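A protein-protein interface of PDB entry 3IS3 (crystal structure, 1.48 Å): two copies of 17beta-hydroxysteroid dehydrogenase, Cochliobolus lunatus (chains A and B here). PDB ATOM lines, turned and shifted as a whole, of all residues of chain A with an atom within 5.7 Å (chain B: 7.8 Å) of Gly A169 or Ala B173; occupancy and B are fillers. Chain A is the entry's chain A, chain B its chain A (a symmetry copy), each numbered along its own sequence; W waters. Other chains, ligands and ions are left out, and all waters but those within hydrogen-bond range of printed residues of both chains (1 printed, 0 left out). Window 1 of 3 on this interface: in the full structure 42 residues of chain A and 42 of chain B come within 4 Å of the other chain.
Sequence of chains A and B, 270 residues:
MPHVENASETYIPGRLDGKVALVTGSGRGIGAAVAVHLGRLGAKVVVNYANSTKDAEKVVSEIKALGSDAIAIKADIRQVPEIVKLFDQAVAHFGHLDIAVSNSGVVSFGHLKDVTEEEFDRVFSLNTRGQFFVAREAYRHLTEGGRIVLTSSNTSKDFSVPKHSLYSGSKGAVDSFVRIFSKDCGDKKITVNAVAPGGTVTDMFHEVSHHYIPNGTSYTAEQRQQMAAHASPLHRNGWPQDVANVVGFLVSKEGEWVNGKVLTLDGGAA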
ATOM      1  N   PHE A 124      -5.060  10.860  -8.094  1.00  0.00           N
ATOM      2  CA  PHE A 124      -5.525  10.412  -6.780  1.00  0.00           C
ATOM      3  C   PHE A 124      -5.529  11.525  -5.729  1.00  0.00           C
ATOM      4  O   PHE A 124      -6.398  11.533  -4.851  1.00  0.00           O
ATOM      5  CB  PHE A 124      -4.723   9.177  -6.324  1.00  0.00           C
ATOM      6  CG  PHE A 124      -5.398   7.884  -6.681  1.00  0.00           C
ATOM      7  CD1 PHE A 124      -5.468   7.493  -8.021  1.00  0.00           C
ATOM      8  CD2 PHE A 124      -6.015   7.094  -5.709  1.00  0.00           C
ATOM      9  CE1 PHE A 124      -6.153   6.338  -8.404  1.00  0.00           C
ATOM     10  CE2 PHE A 124      -6.693   5.921  -6.089  1.00  0.00           C
ATOM     11  CZ  PHE A 124      -6.761   5.544  -7.420  1.00  0.00           C
ATOM     12  N   THR A 128      -9.507  11.294  -5.003  1.00  0.00           N
ATOM     13  CA  THR A 128      -9.661  10.260  -3.998  1.00  0.00           C
ATOM     14  C   THR A 128      -9.225  10.809  -2.635  1.00  0.00           C
ATOM     15  O   THR A 128     -10.043  10.894  -1.718  1.00  0.00           O
ATOM     16  CB  THR A 128      -8.840   9.027  -4.405  1.00  0.00           C
ATOM     17  OG1 THR A 128      -9.216   8.638  -5.719  1.00  0.00           O
ATOM     18  CG2 THR A 128      -9.090   7.867  -3.426  1.00  0.00           C
ATOM     19  N   HIS A 164      -8.663   3.820 -19.226  1.00  0.00           N
ATOM     20  CA  HIS A 164      -9.240   4.698 -18.232  1.00  0.00           C
ATOM     21  C   HIS A 164      -9.141   4.038 -16.846  1.00  0.00           C
ATOM     22  O   HIS A 164      -9.935   4.319 -15.965  1.00  0.00           O
ATOM     23  CB  HIS A 164     -10.711   4.953 -18.662  1.00  0.00           C
ATOM     24  CG  HIS A 164     -11.362   6.146 -18.048  1.00  0.00           C
ATOM     25  ND1 HIS A 164     -10.760   7.390 -17.965  1.00  0.00           N
ATOM     26  CD2 HIS A 164     -12.637   6.320 -17.612  1.00  0.00           C
ATOM     27  CE1 HIS A 164     -11.630   8.263 -17.482  1.00  0.00           C
ATOM     28  NE2 HIS A 164     -12.780   7.645 -17.283  1.00  0.00           N
ATOM     29  N   SER A 165      -8.086   3.240 -16.652  1.00  0.00           N
ATOM     30  CA  SER A 165      -7.976   2.508 -15.395  1.00  0.00           C
ATOM     31  C   SER A 165      -7.714   3.400 -14.200  1.00  0.00           C
ATOM     32  O   SER A 165      -8.304   3.204 -13.145  1.00  0.00           O
ATOM     33  CB  SER A 165      -6.908   1.418 -15.474  1.00  0.00           C
ATOM     34  OG  SER A 165      -5.606   1.964 -15.608  1.00  0.00           O
ATOM     35  N   LEU A 166      -6.831   4.390 -14.369  1.00  0.00           N
ATOM     36  CA  LEU A 166      -6.454   5.250 -13.249  1.00  0.00           C
ATOM     37  C   LEU A 166      -7.668   6.006 -12.711  1.00  0.00           C
ATOM     38  O   LEU A 166      -7.929   5.999 -11.510  1.00  0.00           O
ATOM     39  CB  LEU A 166      -5.340   6.202 -13.701  1.00  0.00           C
ATOM     40  CG  LEU A 166      -4.857   7.185 -12.665  1.00  0.00           C
ATOM     41  CD1 LEU A 166      -4.162   6.406 -11.502  1.00  0.00           C
ATOM     42  CD2 LEU A 166      -3.870   8.123 -13.335  1.00  0.00           C
ATOM     43  N   TYR A 167      -8.414   6.651 -13.629  1.00  0.00           N
ATOM     44  CA  TYR A 167      -9.560   7.414 -13.191  1.00  0.00           C
ATOM     45  C   TYR A 167     -10.636   6.483 -12.578  1.00  0.00           C
ATOM     46  O   TYR A 167     -11.237   6.813 -11.565  1.00  0.00           O
ATOM     47  CB  TYR A 167     -10.132   8.179 -14.391  1.00  0.00           C
ATOM     48  CG  TYR A 167     -11.335   8.987 -13.998  1.00  0.00           C
ATOM     49  CD1 TYR A 167     -11.192  10.273 -13.500  1.00  0.00           C
ATOM     50  CD2 TYR A 167     -12.622   8.448 -14.069  1.00  0.00           C
ATOM     51  CE1 TYR A 167     -12.319  11.035 -13.093  1.00  0.00           C
ATOM     52  CE2 TYR A 167     -13.745   9.207 -13.679  1.00  0.00           C
ATOM     53  CZ  TYR A 167     -13.584  10.484 -13.202  1.00  0.00           C
ATOM     54  OH  TYR A 167     -14.714  11.184 -12.818  1.00  0.00           O
ATOM     55  N   SER A 168     -10.893   5.363 -13.256  1.00  0.00           N
ATOM     56  CA  SER A 168     -11.930   4.445 -12.801  1.00  0.00           C
ATOM     57  C   SER A 168     -11.642   3.990 -11.373  1.00  0.00           C
ATOM     58  O   SER A 168     -12.548   3.965 -10.533  1.00  0.00           O
ATOM     59  CB  SER A 168     -12.034   3.242 -13.748  1.00  0.00           C
ATOM     60  OG  SER A 168     -12.432   3.639 -15.071  1.00  0.00           O
ATOM     61  N   GLY A 169     -10.383   3.672 -11.104  1.00  0.00           N
ATOM     62  CA  GLY A 169      -9.991   3.287  -9.754  1.00  0.00           C
ATOM     63  C   GLY A 169     -10.073   4.430  -8.763  1.00  0.00           C
ATOM     64  O   GLY A 169     -10.437   4.214  -7.589  1.00  0.00           O
ATOM     65  N   SER A 170      -9.810   5.667  -9.197  1.00  0.00           N
ATOM     66  CA  SER A 170      -9.909   6.773  -8.258  1.00  0.00           C
ATOM     67  C   SER A 170     -11.339   6.926  -7.730  1.00  0.00           C
ATOM     68  O   SER A 170     -11.583   7.351  -6.576  1.00  0.00           O
ATOM     69  CB  SER A 170      -9.415   8.095  -8.916  1.00  0.00           C
ATOM     70  OG  SER A 170     -10.387   8.679  -9.806  1.00  0.00           O
ATOM     71  N   LYS A 171     -12.297   6.556  -8.577  1.00  0.00           N
ATOM     72  CA  LYS A 171     -13.713   6.641  -8.184  1.00  0.00           C
ATOM     73  C   LYS A 171     -14.213   5.370  -7.533  1.00  0.00           C
ATOM     74  O   LYS A 171     -15.082   5.434  -6.673  1.00  0.00           O
ATOM     75  CB  LYS A 171     -14.566   7.084  -9.363  1.00  0.00           C
ATOM     76  CG  LYS A 171     -14.121   8.459  -9.886  1.00  0.00           C
ATOM     77  CD  LYS A 171     -13.974   9.491  -8.761  1.00  0.00           C
ATOM     78  CE  LYS A 171     -13.781  10.904  -9.331  1.00  0.00           C
ATOM     79  NZ  LYS A 171     -14.988  11.462 -10.037  1.00  0.00           N
ATOM     80  N   GLY A 172     -13.657   4.202  -7.869  1.00  0.00           N
ATOM     81  CA  GLY A 172     -13.955   2.953  -7.112  1.00  0.00           C
ATOM     82  C   GLY A 172     -13.642   3.115  -5.638  1.00  0.00           C
ATOM     83  O   GLY A 172     -14.401   2.632  -4.785  1.00  0.00           O
ATOM     84  N   ALA A 173     -12.570   3.836  -5.326  1.00  0.00           N
ATOM     85  CA  ALA A 173     -12.257   4.100  -3.906  1.00  0.00           C
ATOM     86  C   ALA A 173     -13.355   4.915  -3.234  1.00  0.00           C
ATOM     87  O   ALA A 173     -13.749   4.636  -2.114  1.00  0.00           O
ATOM     88  CB  ALA A 173     -10.897   4.852  -3.820  1.00  0.00           C
ATOM     89  N   VAL A 174     -13.847   5.930  -3.932  1.00  0.00           N
ATOM     90  CA  VAL A 174     -14.932   6.789  -3.400  1.00  0.00           C
ATOM     91  C   VAL A 174     -16.175   5.964  -3.101  1.00  0.00           C
ATOM     92  O   VAL A 174     -16.833   6.203  -2.056  1.00  0.00           O
ATOM     93  CB  VAL A 174     -15.252   7.952  -4.392  1.00  0.00           C
ATOM     94  CG1 VAL A 174     -16.460   8.747  -3.921  1.00  0.00           C
ATOM     95  CG2 VAL A 174     -14.036   8.868  -4.479  1.00  0.00           C
ATOM     96  N   SER A 176     -16.406   2.843  -2.148  1.00  0.00           N
ATOM     97  CA  SER A 176     -16.216   2.135  -0.895  1.00  0.00           C
ATOM     98  C   SER A 176     -16.191   3.120   0.293  1.00  0.00           C
ATOM     99  O   SER A 176     -16.795   2.851   1.361  1.00  0.00           O
ATOM    100  CB  SER A 176     -14.931   1.353  -0.958  1.00  0.00           C
ATOM    101  OG  SER A 176     -15.036   0.320  -1.933  1.00  0.00           O
ATOM    102  N   PHE B 124      -2.541   4.147   1.092  1.00  0.00           N
ATOM    103  CA  PHE B 124      -2.722   4.163  -0.361  1.00  0.00           C
ATOM    104  C   PHE B 124      -1.422   3.917  -1.133  1.00  0.00           C
ATOM    105  O   PHE B 124      -1.456   3.304  -2.206  1.00  0.00           O
ATOM    106  CB  PHE B 124      -3.425   5.463  -0.796  1.00  0.00           C
ATOM    107  CG  PHE B 124      -4.915   5.306  -0.905  1.00  0.00           C
ATOM    108  CD1 PHE B 124      -5.676   5.141   0.256  1.00  0.00           C
ATOM    109  CD2 PHE B 124      -5.552   5.256  -2.147  1.00  0.00           C
ATOM    110  CE1 PHE B 124      -7.051   4.915   0.195  1.00  0.00           C
ATOM    111  CE2 PHE B 124      -6.940   5.045  -2.213  1.00  0.00           C
ATOM    112  CZ  PHE B 124      -7.685   4.878  -1.056  1.00  0.00           C
ATOM    113  N   ASN B 127      -1.197  -0.185  -0.844  1.00  0.00           N
ATOM    114  CA  ASN B 127      -2.368  -0.985  -1.212  1.00  0.00           C
ATOM    115  C   ASN B 127      -2.909  -0.666  -2.599  1.00  0.00           C
ATOM    116  O   ASN B 127      -3.503  -1.524  -3.245  1.00  0.00           O
ATOM    117  CB  ASN B 127      -3.516  -0.706  -0.238  1.00  0.00           C
ATOM    118  CG  ASN B 127      -3.246  -1.215   1.156  1.00  0.00           C
ATOM    119  OD1 ASN B 127      -2.112  -1.542   1.486  1.00  0.00           O
ATOM    120  ND2 ASN B 127      -4.279  -1.243   1.997  1.00  0.00           N
ATOM    121  N   THR B 128      -2.764   0.586  -3.005  1.00  0.00           N
ATOM    122  CA  THR B 128      -3.452   1.054  -4.191  1.00  0.00           C
ATOM    123  C   THR B 128      -2.421   1.489  -5.239  1.00  0.00           C
ATOM    124  O   THR B 128      -2.356   0.898  -6.318  1.00  0.00           O
ATOM    125  CB  THR B 128      -4.397   2.204  -3.811  1.00  0.00           C
ATOM    126  OG1 THR B 128      -5.251   1.769  -2.762  1.00  0.00           O
ATOM    127  CG2 THR B 128      -5.240   2.633  -5.025  1.00  0.00           C
ATOM    128  N   ARG B 129      -1.583   2.464  -4.895  1.00  0.00           N
ATOM    129  CA  ARG B 129      -0.524   2.916  -5.806  1.00  0.00           C
ATOM    130  C   ARG B 129       0.492   1.809  -6.072  1.00  0.00           C
ATOM    131  O   ARG B 129       0.824   1.513  -7.229  1.00  0.00           O
ATOM    132  CB  ARG B 129       0.140   4.155  -5.211  1.00  0.00           C
ATOM    133  CG  ARG B 129       1.052   4.924  -6.192  1.00  0.00           C
ATOM    134  CD  ARG B 129       1.497   6.164  -5.414  1.00  0.00           C
ATOM    135  NE  ARG B 129       2.308   7.115  -6.159  1.00  0.00           N
ATOM    136  CZ  ARG B 129       3.615   6.975  -6.401  1.00  0.00           C
ATOM    137  NH1 ARG B 129       4.308   5.890  -6.010  1.00  0.00           N
ATOM    138  NH2 ARG B 129       4.234   7.965  -7.044  1.00  0.00           N
ATOM    139  N   PHE B 132      -1.018  -0.861  -8.276  1.00  0.00           N
ATOM    140  CA  PHE B 132      -1.218  -0.315  -9.636  1.00  0.00           C
ATOM    141  C   PHE B 132       0.093  -0.463 -10.398  1.00  0.00           C
ATOM    142  O   PHE B 132       0.108  -0.924 -11.545  1.00  0.00           O
ATOM    143  CB  PHE B 132      -1.584   1.164  -9.546  1.00  0.00           C
ATOM    144  CG  PHE B 132      -1.831   1.803 -10.879  1.00  0.00           C
ATOM    145  CD1 PHE B 132      -0.773   2.256 -11.672  1.00  0.00           C
ATOM    146  CD2 PHE B 132      -3.139   1.909 -11.368  1.00  0.00           C
ATOM    147  CE1 PHE B 132      -0.989   2.846 -12.913  1.00  0.00           C
ATOM    148  CE2 PHE B 132      -3.367   2.500 -12.613  1.00  0.00           C
ATOM    149  CZ  PHE B 132      -2.289   2.959 -13.396  1.00  0.00           C
ATOM    150  N   LEU B 150      -4.141  -9.250  -8.474  1.00  0.00           N
ATOM    151  CA  LEU B 150      -3.952  -8.288  -7.370  1.00  0.00           C
ATOM    152  C   LEU B 150      -4.812  -8.657  -6.173  1.00  0.00           C
ATOM    153  O   LEU B 150      -5.694  -9.526  -6.293  1.00  0.00           O
ATOM    154  CB  LEU B 150      -4.270  -6.871  -7.821  1.00  0.00           C
ATOM    155  CG  LEU B 150      -3.518  -6.382  -9.061  1.00  0.00           C
ATOM    156  CD1 LEU B 150      -3.910  -4.926  -9.285  1.00  0.00           C
ATOM    157  CD2 LEU B 150      -1.976  -6.519  -8.937  1.00  0.00           C
ATOM    158  N   SER B 152      -7.586  -7.502  -3.431  1.00  0.00           N
ATOM    159  CA  SER B 152      -8.601  -6.591  -2.953  1.00  0.00           C
ATOM    160  C   SER B 152      -8.944  -7.008  -1.507  1.00  0.00           C
ATOM    161  O   SER B 152      -8.020  -7.262  -0.738  1.00  0.00           O
ATOM    162  CB  SER B 152      -9.799  -6.641  -3.915  1.00  0.00           C
ATOM    163  OG  SER B 152     -10.847  -5.844  -3.386  1.00  0.00           O
ATOM    164  N   SER B 156     -13.985  -4.302   0.494  1.00  0.00           N
ATOM    165  CA  SER B 156     -14.135  -3.327  -0.589  1.00  0.00           C
ATOM    166  C   SER B 156     -15.628  -3.101  -0.856  1.00  0.00           C
ATOM    167  O   SER B 156     -16.091  -1.950  -0.934  1.00  0.00           O
ATOM    168  CB  SER B 156     -13.433  -3.830  -1.843  1.00  0.00           C
ATOM    169  OG  SER B 156     -13.867  -3.042  -2.927  1.00  0.00           O
ATOM    170  N   LYS B 157     -16.380  -4.192  -0.969  1.00  0.00           N
ATOM    171  CA  LYS B 157     -17.787  -4.137  -1.369  1.00  0.00           C
ATOM    172  C   LYS B 157     -18.692  -5.023  -0.529  1.00  0.00           C
ATOM    173  O   LYS B 157     -19.870  -4.703  -0.352  1.00  0.00           O
ATOM    174  CB  LYS B 157     -17.918  -4.617  -2.826  1.00  0.00           C
ATOM    175  CG  LYS B 157     -17.386  -3.583  -3.821  1.00  0.00           C
ATOM    176  CD  LYS B 157     -17.438  -4.122  -5.277  1.00  0.00           C
ATOM    177  CE  LYS B 157     -16.838  -3.080  -6.234  1.00  0.00           C
ATOM    178  NZ  LYS B 157     -15.623  -2.315  -5.692  1.00  0.00           N
ATOM    179  N   TYR B 167      -9.040   1.756   4.505  1.00  0.00           N
ATOM    180  CA  TYR B 167      -8.617   0.508   3.912  1.00  0.00           C
ATOM    181  C   TYR B 167      -9.638   0.035   2.847  1.00  0.00           C
ATOM    182  O   TYR B 167      -9.254  -0.440   1.787  1.00  0.00           O
ATOM    183  CB  TYR B 167      -8.470  -0.541   5.020  1.00  0.00           C
ATOM    184  CG  TYR B 167      -8.039  -1.867   4.460  1.00  0.00           C
ATOM    185  CD1 TYR B 167      -6.695  -2.157   4.282  1.00  0.00           C
ATOM    186  CD2 TYR B 167      -8.978  -2.819   4.052  1.00  0.00           C
ATOM    187  CE1 TYR B 167      -6.276  -3.393   3.723  1.00  0.00           C
ATOM    188  CE2 TYR B 167      -8.564  -4.053   3.509  1.00  0.00           C
ATOM    189  CZ  TYR B 167      -7.228  -4.327   3.355  1.00  0.00           C
ATOM    190  OH  TYR B 167      -6.872  -5.545   2.805  1.00  0.00           O
ATOM    191  N   SER B 168     -10.924   0.121   3.192  1.00  0.00           N
ATOM    192  CA  SER B 168     -11.965  -0.353   2.290  1.00  0.00           C
ATOM    193  C   SER B 168     -11.865   0.362   0.945  1.00  0.00           C
ATOM    194  O   SER B 168     -11.951  -0.278  -0.109  1.00  0.00           O
ATOM    195  CB  SER B 168     -13.352  -0.149   2.916  1.00  0.00           C
ATOM    196  OG  SER B 168     -13.512  -0.919   4.118  1.00  0.00           O
ATOM    197  N   GLY B 169     -11.647   1.670   0.994  1.00  0.00           N
ATOM    198  CA  GLY B 169     -11.470   2.435  -0.233  1.00  0.00           C
ATOM    199  C   GLY B 169     -10.189   2.095  -0.966  1.00  0.00           C
ATOM    200  O   GLY B 169     -10.167   2.083  -2.214  1.00  0.00           O
ATOM    201  N   SER B 170      -9.116   1.754  -0.244  1.00  0.00           N
ATOM    202  CA  SER B 170      -7.888   1.404  -0.940  1.00  0.00           C
ATOM    203  C   SER B 170      -8.082   0.163  -1.818  1.00  0.00           C
ATOM    204  O   SER B 170      -7.451  -0.003  -2.888  1.00  0.00           O
ATOM    205  CB  SER B 170      -6.727   1.191   0.074  1.00  0.00           C
ATOM    206  OG  SER B 170      -6.787  -0.085   0.742  1.00  0.00           O
ATOM    207  N   LYS B 171      -8.981  -0.711  -1.370  1.00  0.00           N
ATOM    208  CA  LYS B 171      -9.270  -1.938  -2.131  1.00  0.00           C
ATOM    209  C   LYS B 171     -10.390  -1.752  -3.130  1.00  0.00           C
ATOM    210  O   LYS B 171     -10.378  -2.390  -4.176  1.00  0.00           O
ATOM    211  CB  LYS B 171      -9.501  -3.107  -1.185  1.00  0.00           C
ATOM    212  CG  LYS B 171      -8.269  -3.359  -0.301  1.00  0.00           C
ATOM    213  CD  LYS B 171      -6.970  -3.423  -1.115  1.00  0.00           C
ATOM    214  CE  LYS B 171      -5.804  -3.924  -0.252  1.00  0.00           C
ATOM    215  NZ  LYS B 171      -5.914  -5.365   0.170  1.00  0.00           N
ATOM    216  N   GLY B 172     -11.345  -0.852  -2.881  1.00  0.00           N
ATOM    217  CA  GLY B 172     -12.348  -0.474  -3.917  1.00  0.00           C
ATOM    218  C   GLY B 172     -11.672   0.026  -5.179  1.00  0.00           C
ATOM    219  O   GLY B 172     -12.116  -0.296  -6.291  1.00  0.00           O
ATOM    220  N   ALA B 173     -10.574   0.759  -5.024  1.00  0.00           N
ATOM    221  CA  ALA B 173      -9.823   1.208  -6.214  1.00  0.00           C
ATOM    222  C   ALA B 173      -9.269   0.028  -7.003  1.00  0.00           C
ATOM    223  O   ALA B 173      -9.330   0.003  -8.222  1.00  0.00           O
ATOM    224  CB  ALA B 173      -8.665   2.142  -5.758  1.00  0.00           C
ATOM    225  N   VAL B 174      -8.727  -0.953  -6.295  1.00  0.00           N
ATOM    226  CA  VAL B 174      -8.170  -2.166  -6.940  1.00  0.00           C
ATOM    227  C   VAL B 174      -9.244  -2.893  -7.738  1.00  0.00           C
ATOM    228  O   VAL B 174      -8.950  -3.376  -8.862  1.00  0.00           O
ATOM    229  CB  VAL B 174      -7.522  -3.109  -5.878  1.00  0.00           C
ATOM    230  CG1 VAL B 174      -7.082  -4.418  -6.514  1.00  0.00           C
ATOM    231  CG2 VAL B 174      -6.316  -2.403  -5.269  1.00  0.00           C
ATOM    232  N   ASP B 175     -10.469  -2.989  -7.225  1.00  0.00           N
ATOM    233  CA  ASP B 175     -11.528  -3.693  -7.960  1.00  0.00           C
ATOM    234  C   ASP B 175     -11.779  -3.012  -9.309  1.00  0.00           C
ATOM    235  O   ASP B 175     -11.946  -3.704 -10.335  1.00  0.00           O
ATOM    236  CB  ASP B 175     -12.865  -3.717  -7.190  1.00  0.00           C
ATOM    237  CG  ASP B 175     -12.833  -4.481  -5.912  1.00  0.00           C
ATOM    238  OD1 ASP B 175     -11.845  -5.156  -5.641  1.00  0.00           O
ATOM    239  OD2 ASP B 175     -13.870  -4.374  -5.179  1.00  0.00           O
ATOM    240  N   SER B 176     -11.844  -1.667  -9.301  1.00  0.00           N
ATOM    241  CA  SER B 176     -12.053  -0.973 -10.559  1.00  0.00           C
ATOM    242  C   SER B 176     -10.820  -1.115 -11.476  1.00  0.00           C
ATOM    243  O   SER B 176     -10.957  -1.343 -12.703  1.00  0.00           O
ATOM    244  CB  SER B 176     -12.338   0.479 -10.280  1.00  0.00           C
ATOM    245  OG  SER B 176     -13.580   0.609  -9.595  1.00  0.00           O
ATOM    246  N   PHE B 177      -9.613  -0.988 -10.898  1.00  0.00           N
ATOM    247  CA  PHE B 177      -8.402  -1.159 -11.689  1.00  0.00           C
ATOM    248  C   PHE B 177      -8.449  -2.462 -12.478  1.00  0.00           C
ATOM    249  O   PHE B 177      -8.140  -2.478 -13.661  1.00  0.00           O
ATOM    250  CB  PHE B 177      -7.145  -1.232 -10.795  1.00  0.00           C
ATOM    251  CG  PHE B 177      -6.695   0.083 -10.166  1.00  0.00           C
ATOM    252  CD1 PHE B 177      -7.010   1.358 -10.686  1.00  0.00           C
ATOM    253  CD2 PHE B 177      -5.840  -0.002  -9.079  1.00  0.00           C
ATOM    254  CE1 PHE B 177      -6.529   2.539 -10.051  1.00  0.00           C
ATOM    255  CE2 PHE B 177      -5.336   1.153  -8.445  1.00  0.00           C
ATOM    256  CZ  PHE B 177      -5.701   2.421  -8.914  1.00  0.00           C
ATOM    257  N   VAL B 178      -8.732  -3.597 -11.811  1.00  0.00           N
ATOM    258  CA  VAL B 178      -8.557  -4.869 -12.531  1.00  0.00           C
ATOM    259  C   VAL B 178      -9.521  -4.998 -13.700  1.00  0.00           C
ATOM    260  O   VAL B 178      -9.174  -5.568 -14.737  1.00  0.00           O
ATOM    261  CB  VAL B 178      -8.584  -6.142 -11.639  1.00  0.00           C
ATOM    262  CG1 VAL B 178      -7.420  -6.069 -10.615  1.00  0.00           C
ATOM    263  CG2 VAL B 178      -9.900  -6.332 -10.972  1.00  0.00           C
ATOM    264  N   ARG B 179     -10.747  -4.483 -13.533  1.00  0.00           N
ATOM    265  CA  ARG B 179     -11.716  -4.545 -14.625  1.00  0.00           C
ATOM    266  C   ARG B 179     -11.189  -3.807 -15.872  1.00  0.00           C
ATOM    267  O   ARG B 179     -11.334  -4.276 -16.997  1.00  0.00           O
ATOM    268  CB  ARG B 179     -13.048  -3.954 -14.195  1.00  0.00           C
ATOM    269  CG  ARG B 179     -14.156  -4.289 -15.180  1.00  0.00           C
ATOM    270  CD  ARG B 179     -15.504  -3.747 -14.725  1.00  0.00           C
ATOM    271  NE  ARG B 179     -15.648  -2.306 -14.971  1.00  0.00           N
ATOM    272  CZ  ARG B 179     -15.487  -1.357 -14.052  1.00  0.00           C
ATOM    273  NH1 ARG B 179     -15.175  -1.652 -12.791  1.00  0.00           N
ATOM    274  NH2 ARG B 179     -15.689  -0.078 -14.398  1.00  0.00           N
ATOM    275  N   ILE B 180     -10.544  -2.671 -15.659  1.00  0.00           N
ATOM    276  CA  ILE B 180     -10.071  -1.898 -16.805  1.00  0.00           C
ATOM    277  C   ILE B 180      -8.695  -2.399 -17.263  1.00  0.00           C
ATOM    278  O   ILE B 180      -8.399  -2.395 -18.479  1.00  0.00           O
ATOM    279  CB  ILE B 180     -10.042  -0.397 -16.502  1.00  0.00           C
ATOM    280  CG1 ILE B 180     -11.410   0.097 -15.958  1.00  0.00           C
ATOM    281  CG2 ILE B 180      -9.626   0.399 -17.757  1.00  0.00           C
ATOM    282  CD1 ILE B 180     -12.629  -0.361 -16.790  1.00  0.00           C
ATOM    283  N   PHE B 181      -7.847  -2.818 -16.308  1.00  0.00           N
ATOM    284  CA  PHE B 181      -6.560  -3.424 -16.708  1.00  0.00           C
ATOM    285  C   PHE B 181      -6.783  -4.575 -17.640  1.00  0.00           C
ATOM    286  O   PHE B 181      -5.987  -4.806 -18.551  1.00  0.00           O
ATOM    287  CB  PHE B 181      -5.830  -3.985 -15.482  1.00  0.00           C
ATOM    288  CG  PHE B 181      -5.228  -2.945 -14.550  1.00  0.00           C
ATOM    289  CD1 PHE B 181      -5.250  -1.611 -14.963  1.00  0.00           C
ATOM    290  CD2 PHE B 181      -4.682  -3.268 -13.301  1.00  0.00           C
ATOM    291  CE1 PHE B 181      -4.742  -0.600 -14.168  1.00  0.00           C
ATOM    292  CE2 PHE B 181      -4.155  -2.241 -12.468  1.00  0.00           C
ATOM    293  CZ  PHE B 181      -4.211  -0.910 -12.904  1.00  0.00           C
HETATM  294  O   HOH W   1     -16.532  -0.154  -4.161  1.00  0.00           O
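Of chain B, only Ala B173, Ser B176 and Phe B177 come within 4 Å of Gly A169. Printed residues of chain A within 4 Å of Ser B156: Ser A176. Of the printed residues of chain A, Ser B168 touches Ser A176 (3.5 Å). Lys B171 touches none of the printed residues of chain A. Of chain A, only Gly A169 (3.3 Å), Gly A172 (3.9 Å) and Ala A173 (3.7 Å) come within 4 Å of Ala B173. Of the printed residues of chain A, Ser B176 touches Ser A168, Gly A169 and Gly A172. The nearest residue of chain A that does not touch Ala B173 is Phe A124 (4.2 Å).
Water W1 bridges OG of Ser A176 and NZ of Lys B157.
OG of Ser A176 lies within hydrogen-bond range of O of Ser B156, 2.7 Å away.
Phe A124 touches Thr B128, and with the chains exchanged Thr A128 touches Phe B124. Gly B172 touches its own counterpart, Gly A172. Gly A172 touches Ser B176, and with the chains exchanged Ser A176 touches Gly B172. Ala B173 touches its own counterpart, Ala A173.
Of the 14 printed residues of chain A, 9 touch a printed residue of chain B. Hydrophobic or aromatic side chains of chain A that line the printed part of chain B: Phe A124 and Ala A173. Among the printed residues, no Asp or Glu carboxylate lies within 4 Å of a Lys or Arg side-chain nitrogen of the other chain.
The backbone carbonyl oxygen (O) of Ser A170 lies within hydrogen-bond range of the side-chain hydroxyl (OG1) of Thr A128 (2.8 Å). The backbone carbonyl oxygen (O) of His A164 sits at hydrogen-bond distance from the side-chain hydroxyl (OG) of Ser A168 (2.7 Å). O of Phe B124 lies within hydrogen-bond range of N of Arg B129 (2.8 Å). The side-chain hydroxyl of Ser B156 sits at hydrogen-bond distance from the side-chain amino group of Lys B157, 3.4 Å away. The side-chain hydroxyl (OG) of Ser B156 lies close to the backbone NH (N) of Gly B172 (3.3 Å). The side-chain hydroxyl of Ser B156 sits at hydrogen-bond distance from the side-chain carboxylate of Asp B175, 2.6 Å away.
Among the printed residues, merely in contact across the chains: Phe A124 with Phe B124, Phe A124 with Thr B128, Phe A124 with Phe B177, Thr A128 with Phe B124, His A164 with Ile B180, Ser A165 with Phe B132, Ser A165 with Phe B177, Ser A165 with Ile B180, Ser A165 with Phe B181, Ser A168 with Ser B176, Ser A168 with Ile B180, Gly A169 with Ala B173, Gly A169 with Ser B176, Gly A169 with Phe B177, Gly A172 with Gly B172, Gly A172 with Ala B173, Gly A172 with Ser B176, Ala A173 with Gly B169, Ala A173 with Gly B172, Ala A173 with Ala B173, Ser A176 with Ser B168, Ser A176 with Gly B169 and Ser A176 with Gly B172.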
